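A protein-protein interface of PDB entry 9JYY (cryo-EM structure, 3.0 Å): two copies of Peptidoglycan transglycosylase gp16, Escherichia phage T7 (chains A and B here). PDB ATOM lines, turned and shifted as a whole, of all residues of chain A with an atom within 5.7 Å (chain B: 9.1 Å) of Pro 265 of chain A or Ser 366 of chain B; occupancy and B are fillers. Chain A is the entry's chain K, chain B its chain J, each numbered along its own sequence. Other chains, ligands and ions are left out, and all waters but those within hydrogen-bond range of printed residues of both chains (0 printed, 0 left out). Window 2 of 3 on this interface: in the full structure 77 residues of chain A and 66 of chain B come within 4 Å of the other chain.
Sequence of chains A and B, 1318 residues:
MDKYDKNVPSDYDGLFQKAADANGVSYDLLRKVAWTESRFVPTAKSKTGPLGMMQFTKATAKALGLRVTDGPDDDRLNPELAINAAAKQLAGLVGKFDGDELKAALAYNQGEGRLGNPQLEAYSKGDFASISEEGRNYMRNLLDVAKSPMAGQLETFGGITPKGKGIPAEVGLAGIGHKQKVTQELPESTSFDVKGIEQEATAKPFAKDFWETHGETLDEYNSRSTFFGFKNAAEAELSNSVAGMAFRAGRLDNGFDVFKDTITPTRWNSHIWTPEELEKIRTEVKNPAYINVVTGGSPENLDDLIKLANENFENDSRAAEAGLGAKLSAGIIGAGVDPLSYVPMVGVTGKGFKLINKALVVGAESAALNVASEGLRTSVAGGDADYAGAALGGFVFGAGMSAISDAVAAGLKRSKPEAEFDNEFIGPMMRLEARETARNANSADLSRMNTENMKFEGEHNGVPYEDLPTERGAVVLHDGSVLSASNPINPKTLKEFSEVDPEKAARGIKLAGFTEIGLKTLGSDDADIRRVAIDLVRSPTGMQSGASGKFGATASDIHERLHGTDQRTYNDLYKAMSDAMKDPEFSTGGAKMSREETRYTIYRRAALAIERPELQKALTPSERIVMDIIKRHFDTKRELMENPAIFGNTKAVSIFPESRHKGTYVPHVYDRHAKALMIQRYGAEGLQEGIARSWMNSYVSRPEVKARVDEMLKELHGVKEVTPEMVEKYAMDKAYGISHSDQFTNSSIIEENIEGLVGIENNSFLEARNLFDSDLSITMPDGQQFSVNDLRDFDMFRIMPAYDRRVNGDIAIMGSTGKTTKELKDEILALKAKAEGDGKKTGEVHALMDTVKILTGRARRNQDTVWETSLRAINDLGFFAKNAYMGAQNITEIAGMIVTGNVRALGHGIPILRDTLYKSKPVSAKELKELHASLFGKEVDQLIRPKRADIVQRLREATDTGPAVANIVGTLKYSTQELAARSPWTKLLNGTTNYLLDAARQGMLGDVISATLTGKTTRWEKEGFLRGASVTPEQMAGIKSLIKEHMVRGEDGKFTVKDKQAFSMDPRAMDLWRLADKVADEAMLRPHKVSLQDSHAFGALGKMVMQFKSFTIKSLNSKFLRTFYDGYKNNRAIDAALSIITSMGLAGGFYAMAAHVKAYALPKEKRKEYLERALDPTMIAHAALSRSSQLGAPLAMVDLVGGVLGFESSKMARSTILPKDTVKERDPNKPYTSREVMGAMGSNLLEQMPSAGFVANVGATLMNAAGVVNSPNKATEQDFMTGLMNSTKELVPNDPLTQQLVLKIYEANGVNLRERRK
OG of Ser 366 of chain B lies within hydrogen-bond range of O of Pro 265 of chain A. The backbone carbonyl oxygen (O) of Ser 270 of chain A sits close to the side-chain carboxylate (OE2) of Glu 374 of chain B (3.0 Å).
Of chain B, only Ser 366 and Ala 367 come within 4 Å of Pro 265 of chain A. Of chain A, only Pro 265, Thr 266 and Arg 267 come within 4 Å of Ser 366 of chain B. Printed residues of chain A within 4 Å of Glu 374 of chain B: Ser 270 (3.0 Å). Printed residues of chain B within 4 Å of Ser 270 of chain A: Ala 367 and Glu 374. Of the printed residues of chain A, Ala 367 of chain B touches Pro 265 and Ser 270. Of the printed residues of chain B, Arg 267 of chain A touches Ser 366. Tyr 1125 of chain A touches none of the printed residues of chain B. Ala 364 of chain B touches none of the printed residues of chain A. The nearest residue of chain B that does not touch Pro 265 of chain A is Glu 365 of chain B (6.2 Å). The nearest printed residue of chain B that does not touch Ser 270 of chain A is Ala 368 of chain B (4.6 Å).
No position is printed for both chains.
Hydrophobic or aromatic side chains of chain B that line the printed part of chain A: Ala 367. Along chain B the printed residues that touch a printed residue of chain A span positions 366 to 374. Of the 11 printed residues of chain A, 4 touch a printed residue of chain B. Hydrophobic or aromatic side chains of chain A within 4 Å of the printed part of chain B: Pro 265. Among the printed residues, no Asp or Glu carboxylate lies within 4 Å of a Lys or Arg side-chain nitrogen of the other chain.
CB of Pro 265 of chain A touches CB of Ala 367 of chain B, 3.6 Å away. Thr 266 of chain A touches Ser 366 of chain B. Ser 366 of chain B touches Arg 267 of chain A. Ala 367 of chain B touches Ser 270 of chain A.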
ATOM      1  N   PHE A 259     -17.109   7.621  -4.447  1.00  0.00           N
ATOM      2  CA  PHE A 259     -17.764   8.732  -5.125  1.00  0.00           C
ATOM      3  C   PHE A 259     -16.783   9.850  -5.444  1.00  0.00           C
ATOM      4  O   PHE A 259     -17.103  10.758  -6.217  1.00  0.00           O
ATOM      5  CB  PHE A 259     -18.934   9.236  -4.290  1.00  0.00           C
ATOM      6  CG  PHE A 259     -20.010   8.216  -4.112  1.00  0.00           C
ATOM      7  CD1 PHE A 259     -20.806   7.851  -5.173  1.00  0.00           C
ATOM      8  CD2 PHE A 259     -20.208   7.605  -2.896  1.00  0.00           C
ATOM      9  CE1 PHE A 259     -21.785   6.910  -5.022  1.00  0.00           C
ATOM     10  CE2 PHE A 259     -21.184   6.662  -2.740  1.00  0.00           C
ATOM     11  CZ  PHE A 259     -21.975   6.313  -3.806  1.00  0.00           C
ATOM     12  N   ILE A 263     -17.134   7.291  -9.110  1.00  0.00           N
ATOM     13  CA  ILE A 263     -18.311   7.950  -9.668  1.00  0.00           C
ATOM     14  C   ILE A 263     -18.419   9.360  -9.118  1.00  0.00           C
ATOM     15  O   ILE A 263     -18.858   9.570  -7.983  1.00  0.00           O
ATOM     16  CB  ILE A 263     -19.590   7.154  -9.379  1.00  0.00           C
ATOM     17  CG1 ILE A 263     -19.663   5.940 -10.289  1.00  0.00           C
ATOM     18  CG2 ILE A 263     -20.817   7.997  -9.636  1.00  0.00           C
ATOM     19  CD1 ILE A 263     -20.705   4.985  -9.869  1.00  0.00           C
ATOM     20  N   THR A 264     -18.007  10.332  -9.914  1.00  0.00           N
ATOM     21  CA  THR A 264     -18.036  11.708  -9.463  1.00  0.00           C
ATOM     22  C   THR A 264     -19.385  12.334  -9.799  1.00  0.00           C
ATOM     23  O   THR A 264     -19.844  12.243 -10.942  1.00  0.00           O
ATOM     24  CB  THR A 264     -16.911  12.504 -10.112  1.00  0.00           C
ATOM     25  OG1 THR A 264     -16.871  12.211 -11.513  1.00  0.00           O
ATOM     26  CG2 THR A 264     -15.587  12.121  -9.489  1.00  0.00           C
ATOM     27  N   PRO A 265     -20.055  12.954  -8.831  1.00  0.00           N
ATOM     28  CA  PRO A 265     -21.300  13.668  -9.127  1.00  0.00           C
ATOM     29  C   PRO A 265     -21.030  14.826 -10.074  1.00  0.00           C
ATOM     30  O   PRO A 265     -20.304  15.760  -9.737  1.00  0.00           O
ATOM     31  CB  PRO A 265     -21.758  14.160  -7.751  1.00  0.00           C
ATOM     32  CG  PRO A 265     -21.082  13.252  -6.787  1.00  0.00           C
ATOM     33  CD  PRO A 265     -19.753  12.966  -7.393  1.00  0.00           C
ATOM     34  N   THR A 266     -21.611  14.759 -11.266  1.00  0.00           N
ATOM     35  CA  THR A 266     -21.468  15.861 -12.197  1.00  0.00           C
ATOM     36  C   THR A 266     -22.442  16.980 -11.840  1.00  0.00           C
ATOM     37  O   THR A 266     -23.160  16.926 -10.841  1.00  0.00           O
ATOM     38  CB  THR A 266     -21.691  15.398 -13.637  1.00  0.00           C
ATOM     39  OG1 THR A 266     -21.554  16.514 -14.522  1.00  0.00           O
ATOM     40  CG2 THR A 266     -23.069  14.838 -13.806  1.00  0.00           C
ATOM     41  N   ARG A 267     -22.446  18.015 -12.675  1.00  0.00           N
ATOM     42  CA  ARG A 267     -23.332  19.148 -12.443  1.00  0.00           C
ATOM     43  C   ARG A 267     -24.783  18.750 -12.668  1.00  0.00           C
ATOM     44  O   ARG A 267     -25.684  19.228 -11.973  1.00  0.00           O
ATOM     45  CB  ARG A 267     -22.925  20.305 -13.361  1.00  0.00           C
ATOM     46  CG  ARG A 267     -23.287  21.717 -12.892  1.00  0.00           C
ATOM     47  CD  ARG A 267     -24.774  22.016 -12.935  1.00  0.00           C
ATOM     48  NE  ARG A 267     -25.043  23.448 -12.955  1.00  0.00           N
ATOM     49  CZ  ARG A 267     -26.244  23.986 -12.793  1.00  0.00           C
ATOM     50  NH1 ARG A 267     -27.310  23.238 -12.576  1.00  0.00           N
ATOM     51  NH2 ARG A 267     -26.377  25.307 -12.856  1.00  0.00           N
ATOM     52  N   ASN A 269     -26.164  15.498 -12.814  1.00  0.00           N
ATOM     53  CA  ASN A 269     -26.593  14.683 -11.692  1.00  0.00           C
ATOM     54  C   ASN A 269     -26.635  15.547 -10.441  1.00  0.00           C
ATOM     55  O   ASN A 269     -26.014  16.609 -10.373  1.00  0.00           O
ATOM     56  CB  ASN A 269     -25.659  13.496 -11.460  1.00  0.00           C
ATOM     57  CG  ASN A 269     -25.476  12.649 -12.689  1.00  0.00           C
ATOM     58  OD1 ASN A 269     -24.383  12.172 -12.972  1.00  0.00           O
ATOM     59  ND2 ASN A 269     -26.550  12.463 -13.438  1.00  0.00           N
ATOM     60  N   SER A 270     -27.388  15.093  -9.450  1.00  0.00           N
ATOM     61  CA  SER A 270     -27.534  15.743  -8.152  1.00  0.00           C
ATOM     62  C   SER A 270     -28.221  17.098  -8.237  1.00  0.00           C
ATOM     63  O   SER A 270     -28.478  17.702  -7.189  1.00  0.00           O
ATOM     64  CB  SER A 270     -26.187  15.931  -7.450  1.00  0.00           C
ATOM     65  OG  SER A 270     -25.415  16.906  -8.128  1.00  0.00           O
ATOM     66  N   PRO A 984     -24.280  10.217  -0.861  1.00  0.00           N
ATOM     67  CA  PRO A 984     -24.146  10.040  -2.311  1.00  0.00           C
ATOM     68  C   PRO A 984     -24.725   8.725  -2.778  1.00  0.00           C
ATOM     69  O   PRO A 984     -25.026   8.574  -3.965  1.00  0.00           O
ATOM     70  CB  PRO A 984     -22.633  10.113  -2.531  1.00  0.00           C
ATOM     71  CG  PRO A 984     -22.127  10.878  -1.378  1.00  0.00           C
ATOM     72  CD  PRO A 984     -22.980  10.466  -0.223  1.00  0.00           C
ATOM     73  N   LEU A 988     -26.849   9.342  -5.846  1.00  0.00           N
ATOM     74  CA  LEU A 988     -26.316   8.564  -6.946  1.00  0.00           C
ATOM     75  C   LEU A 988     -26.596   7.109  -6.616  1.00  0.00           C
ATOM     76  O   LEU A 988     -26.278   6.665  -5.514  1.00  0.00           O
ATOM     77  CB  LEU A 988     -24.809   8.771  -7.067  1.00  0.00           C
ATOM     78  CG  LEU A 988     -24.198  10.160  -7.250  1.00  0.00           C
ATOM     79  CD1 LEU A 988     -22.696  10.047  -7.198  1.00  0.00           C
ATOM     80  CD2 LEU A 988     -24.617  10.835  -8.514  1.00  0.00           C
ATOM     81  N   TYR A1125     -19.216   5.130 -17.366  1.00  0.00           N
ATOM     82  CA  TYR A1125     -19.481   6.349 -16.615  1.00  0.00           C
ATOM     83  C   TYR A1125     -18.588   7.486 -17.085  1.00  0.00           C
ATOM     84  O   TYR A1125     -19.001   8.648 -17.089  1.00  0.00           O
ATOM     85  CB  TYR A1125     -19.301   6.125 -15.119  1.00  0.00           C
ATOM     86  CG  TYR A1125     -19.819   7.302 -14.334  1.00  0.00           C
ATOM     87  CD1 TYR A1125     -21.169   7.447 -14.092  1.00  0.00           C
ATOM     88  CD2 TYR A1125     -18.964   8.296 -13.885  1.00  0.00           C
ATOM     89  CE1 TYR A1125     -21.654   8.526 -13.400  1.00  0.00           C
ATOM     90  CE2 TYR A1125     -19.442   9.380 -13.191  1.00  0.00           C
ATOM     91  CZ  TYR A1125     -20.790   9.492 -12.952  1.00  0.00           C
ATOM     92  OH  TYR A1125     -21.277  10.571 -12.262  1.00  0.00           O
ATOM     93  N   GLY B 363     -11.065  25.590  -5.295  1.00  0.00           N
ATOM     94  CA  GLY B 363     -11.737  24.315  -5.182  1.00  0.00           C
ATOM     95  C   GLY B 363     -13.144  24.573  -5.624  1.00  0.00           C
ATOM     96  O   GLY B 363     -13.656  25.651  -5.363  1.00  0.00           O
ATOM     97  N   ALA B 364     -13.752  23.624  -6.320  1.00  0.00           N
ATOM     98  CA  ALA B 364     -14.840  23.935  -7.231  1.00  0.00           C
ATOM     99  C   ALA B 364     -15.645  22.697  -7.517  1.00  0.00           C
ATOM    100  O   ALA B 364     -15.531  22.111  -8.587  1.00  0.00           O
ATOM    101  CB  ALA B 364     -14.313  24.533  -8.519  1.00  0.00           C
ATOM    102  N   GLU B 365     -16.464  22.289  -6.557  1.00  0.00           N
ATOM    103  CA  GLU B 365     -17.257  21.083  -6.728  1.00  0.00           C
ATOM    104  C   GLU B 365     -18.355  21.316  -7.739  1.00  0.00           C
ATOM    105  O   GLU B 365     -18.827  22.434  -7.890  1.00  0.00           O
ATOM    106  CB  GLU B 365     -17.845  20.623  -5.395  1.00  0.00           C
ATOM    107  CG  GLU B 365     -18.618  21.685  -4.633  1.00  0.00           C
ATOM    108  CD  GLU B 365     -17.834  22.259  -3.474  1.00  0.00           C
ATOM    109  OE1 GLU B 365     -16.628  21.957  -3.364  1.00  0.00           O
ATOM    110  OE2 GLU B 365     -18.422  23.017  -2.676  1.00  0.00           O
ATOM    111  N   SER B 366     -18.742  20.275  -8.461  1.00  0.00           N
ATOM    112  CA  SER B 366     -19.844  20.412  -9.406  1.00  0.00           C
ATOM    113  C   SER B 366     -21.178  20.068  -8.757  1.00  0.00           C
ATOM    114  O   SER B 366     -22.236  20.504  -9.224  1.00  0.00           O
ATOM    115  CB  SER B 366     -19.591  19.528 -10.622  1.00  0.00           C
ATOM    116  OG  SER B 366     -19.281  18.207 -10.220  1.00  0.00           O
ATOM    117  N   ALA B 367     -21.151  19.280  -7.688  1.00  0.00           N
ATOM    118  CA  ALA B 367     -22.365  18.944  -6.961  1.00  0.00           C
ATOM    119  C   ALA B 367     -22.546  19.886  -5.780  1.00  0.00           C
ATOM    120  O   ALA B 367     -21.621  20.087  -4.990  1.00  0.00           O
ATOM    121  CB  ALA B 367     -22.313  17.497  -6.478  1.00  0.00           C
ATOM    122  N   ALA B 368     -23.735  20.465  -5.663  1.00  0.00           N
ATOM    123  CA  ALA B 368     -24.023  21.343  -4.539  1.00  0.00           C
ATOM    124  C   ALA B 368     -24.220  20.533  -3.264  1.00  0.00           C
ATOM    125  O   ALA B 368     -24.597  19.360  -3.306  1.00  0.00           O
ATOM    126  CB  ALA B 368     -25.259  22.186  -4.826  1.00  0.00           C
ATOM    127  N   LEU B 369     -23.957  21.170  -2.124  1.00  0.00           N
ATOM    128  CA  LEU B 369     -24.006  20.464  -0.848  1.00  0.00           C
ATOM    129  C   LEU B 369     -25.416  20.030  -0.480  1.00  0.00           C
ATOM    130  O   LEU B 369     -25.606  18.919   0.026  1.00  0.00           O
ATOM    131  CB  LEU B 369     -23.435  21.344   0.257  1.00  0.00           C
ATOM    132  CG  LEU B 369     -21.929  21.266   0.483  1.00  0.00           C
ATOM    133  CD1 LEU B 369     -21.573  21.970   1.776  1.00  0.00           C
ATOM    134  CD2 LEU B 369     -21.472  19.825   0.500  1.00  0.00           C
ATOM    135  N   ASN B 370     -26.408  20.885  -0.710  1.00  0.00           N
ATOM    136  CA  ASN B 370     -27.782  20.609  -0.323  1.00  0.00           C
ATOM    137  C   ASN B 370     -28.672  20.766  -1.542  1.00  0.00           C
ATOM    138  O   ASN B 370     -28.238  21.220  -2.602  1.00  0.00           O
ATOM    139  CB  ASN B 370     -28.260  21.557   0.779  1.00  0.00           C
ATOM    140  CG  ASN B 370     -27.486  21.403   2.058  1.00  0.00           C
ATOM    141  OD1 ASN B 370     -26.782  22.319   2.478  1.00  0.00           O
ATOM    142  ND2 ASN B 370     -27.605  20.243   2.689  1.00  0.00           N
ATOM    143  N   GLU B 374     -27.703  25.114  -4.374  1.00  0.00           N
ATOM    144  CA  GLU B 374     -27.881  24.837  -5.805  1.00  0.00           C
ATOM    145  C   GLU B 374     -28.037  26.178  -6.510  1.00  0.00           C
ATOM    146  O   GLU B 374     -27.037  26.902  -6.649  1.00  0.00           O
ATOM    147  CB  GLU B 374     -28.997  23.824  -6.078  1.00  0.00           C
ATOM    148  CG  GLU B 374     -28.662  22.403  -5.667  1.00  0.00           C
ATOM    149  CD  GLU B 374     -29.754  21.406  -6.013  1.00  0.00           C
ATOM    150  OE1 GLU B 374     -30.840  21.832  -6.449  1.00  0.00           O
ATOM    151  OE2 GLU B 374     -29.512  20.190  -5.867  1.00  0.00           O
ATOM    152  N   ASN B 440     -21.064  31.098  -9.361  1.00  0.00           N
ATOM    153  CA  ASN B 440     -21.294  30.393 -10.613  1.00  0.00           C
ATOM    154  C   ASN B 440     -20.417  29.153 -10.721  1.00  0.00           C
ATOM    155  O   ASN B 440     -20.781  28.185 -11.397  1.00  0.00           O
ATOM    156  CB  ASN B 440     -21.057  31.341 -11.780  1.00  0.00           C
ATOM    157  CG  ASN B 440     -21.938  32.558 -11.718  1.00  0.00           C
ATOM    158  OD1 ASN B 440     -23.124  32.464 -11.420  1.00  0.00           O
ATOM    159  ND2 ASN B 440     -21.361  33.717 -11.983  1.00  0.00           N
ATOM    160  N   ALA B 441     -19.255  29.162 -10.070  1.00  0.00           N
ATOM    161  CA  ALA B 441     -18.375  28.005 -10.038  1.00  0.00           C
ATOM    162  C   ALA B 441     -18.634  27.097  -8.848  1.00  0.00           C
ATOM    163  O   ALA B 441     -18.044  26.016  -8.775  1.00  0.00           O
ATOM    164  CB  ALA B 441     -16.915  28.456 -10.034  1.00  0.00           C
ATOM    165  N   ASN B 442     -19.494  27.516  -7.924  1.00  0.00           N
ATOM    166  CA  ASN B 442     -20.123  26.758  -6.842  1.00  0.00           C
ATOM    167  C   ASN B 442     -19.160  26.620  -5.655  1.00  0.00           C
ATOM    168  O   ASN B 442     -19.610  26.252  -4.575  1.00  0.00           O
ATOM    169  CB  ASN B 442     -20.617  25.385  -7.359  1.00  0.00           C
ATOM    170  CG  ASN B 442     -21.014  24.372  -6.266  1.00  0.00           C
ATOM    171  OD1 ASN B 442     -21.231  24.692  -5.108  1.00  0.00           O
ATOM    172  ND2 ASN B 442     -21.106  23.116  -6.673  1.00  0.00           N
ATOM    173  N   SER B 443     -17.901  27.039  -5.747  1.00  0.00           N
ATOM    174  CA  SER B 443     -17.100  26.799  -4.554  1.00  0.00           C
ATOM    175  C   SER B 443     -16.004  27.835  -4.362  1.00  0.00           C
ATOM    176  O   SER B 443     -15.514  28.446  -5.315  1.00  0.00           O
ATOM    177  CB  SER B 443     -16.500  25.393  -4.582  1.00  0.00           C
ATOM    178  OG  SER B 443     -16.041  25.002  -3.297  1.00  0.00           O
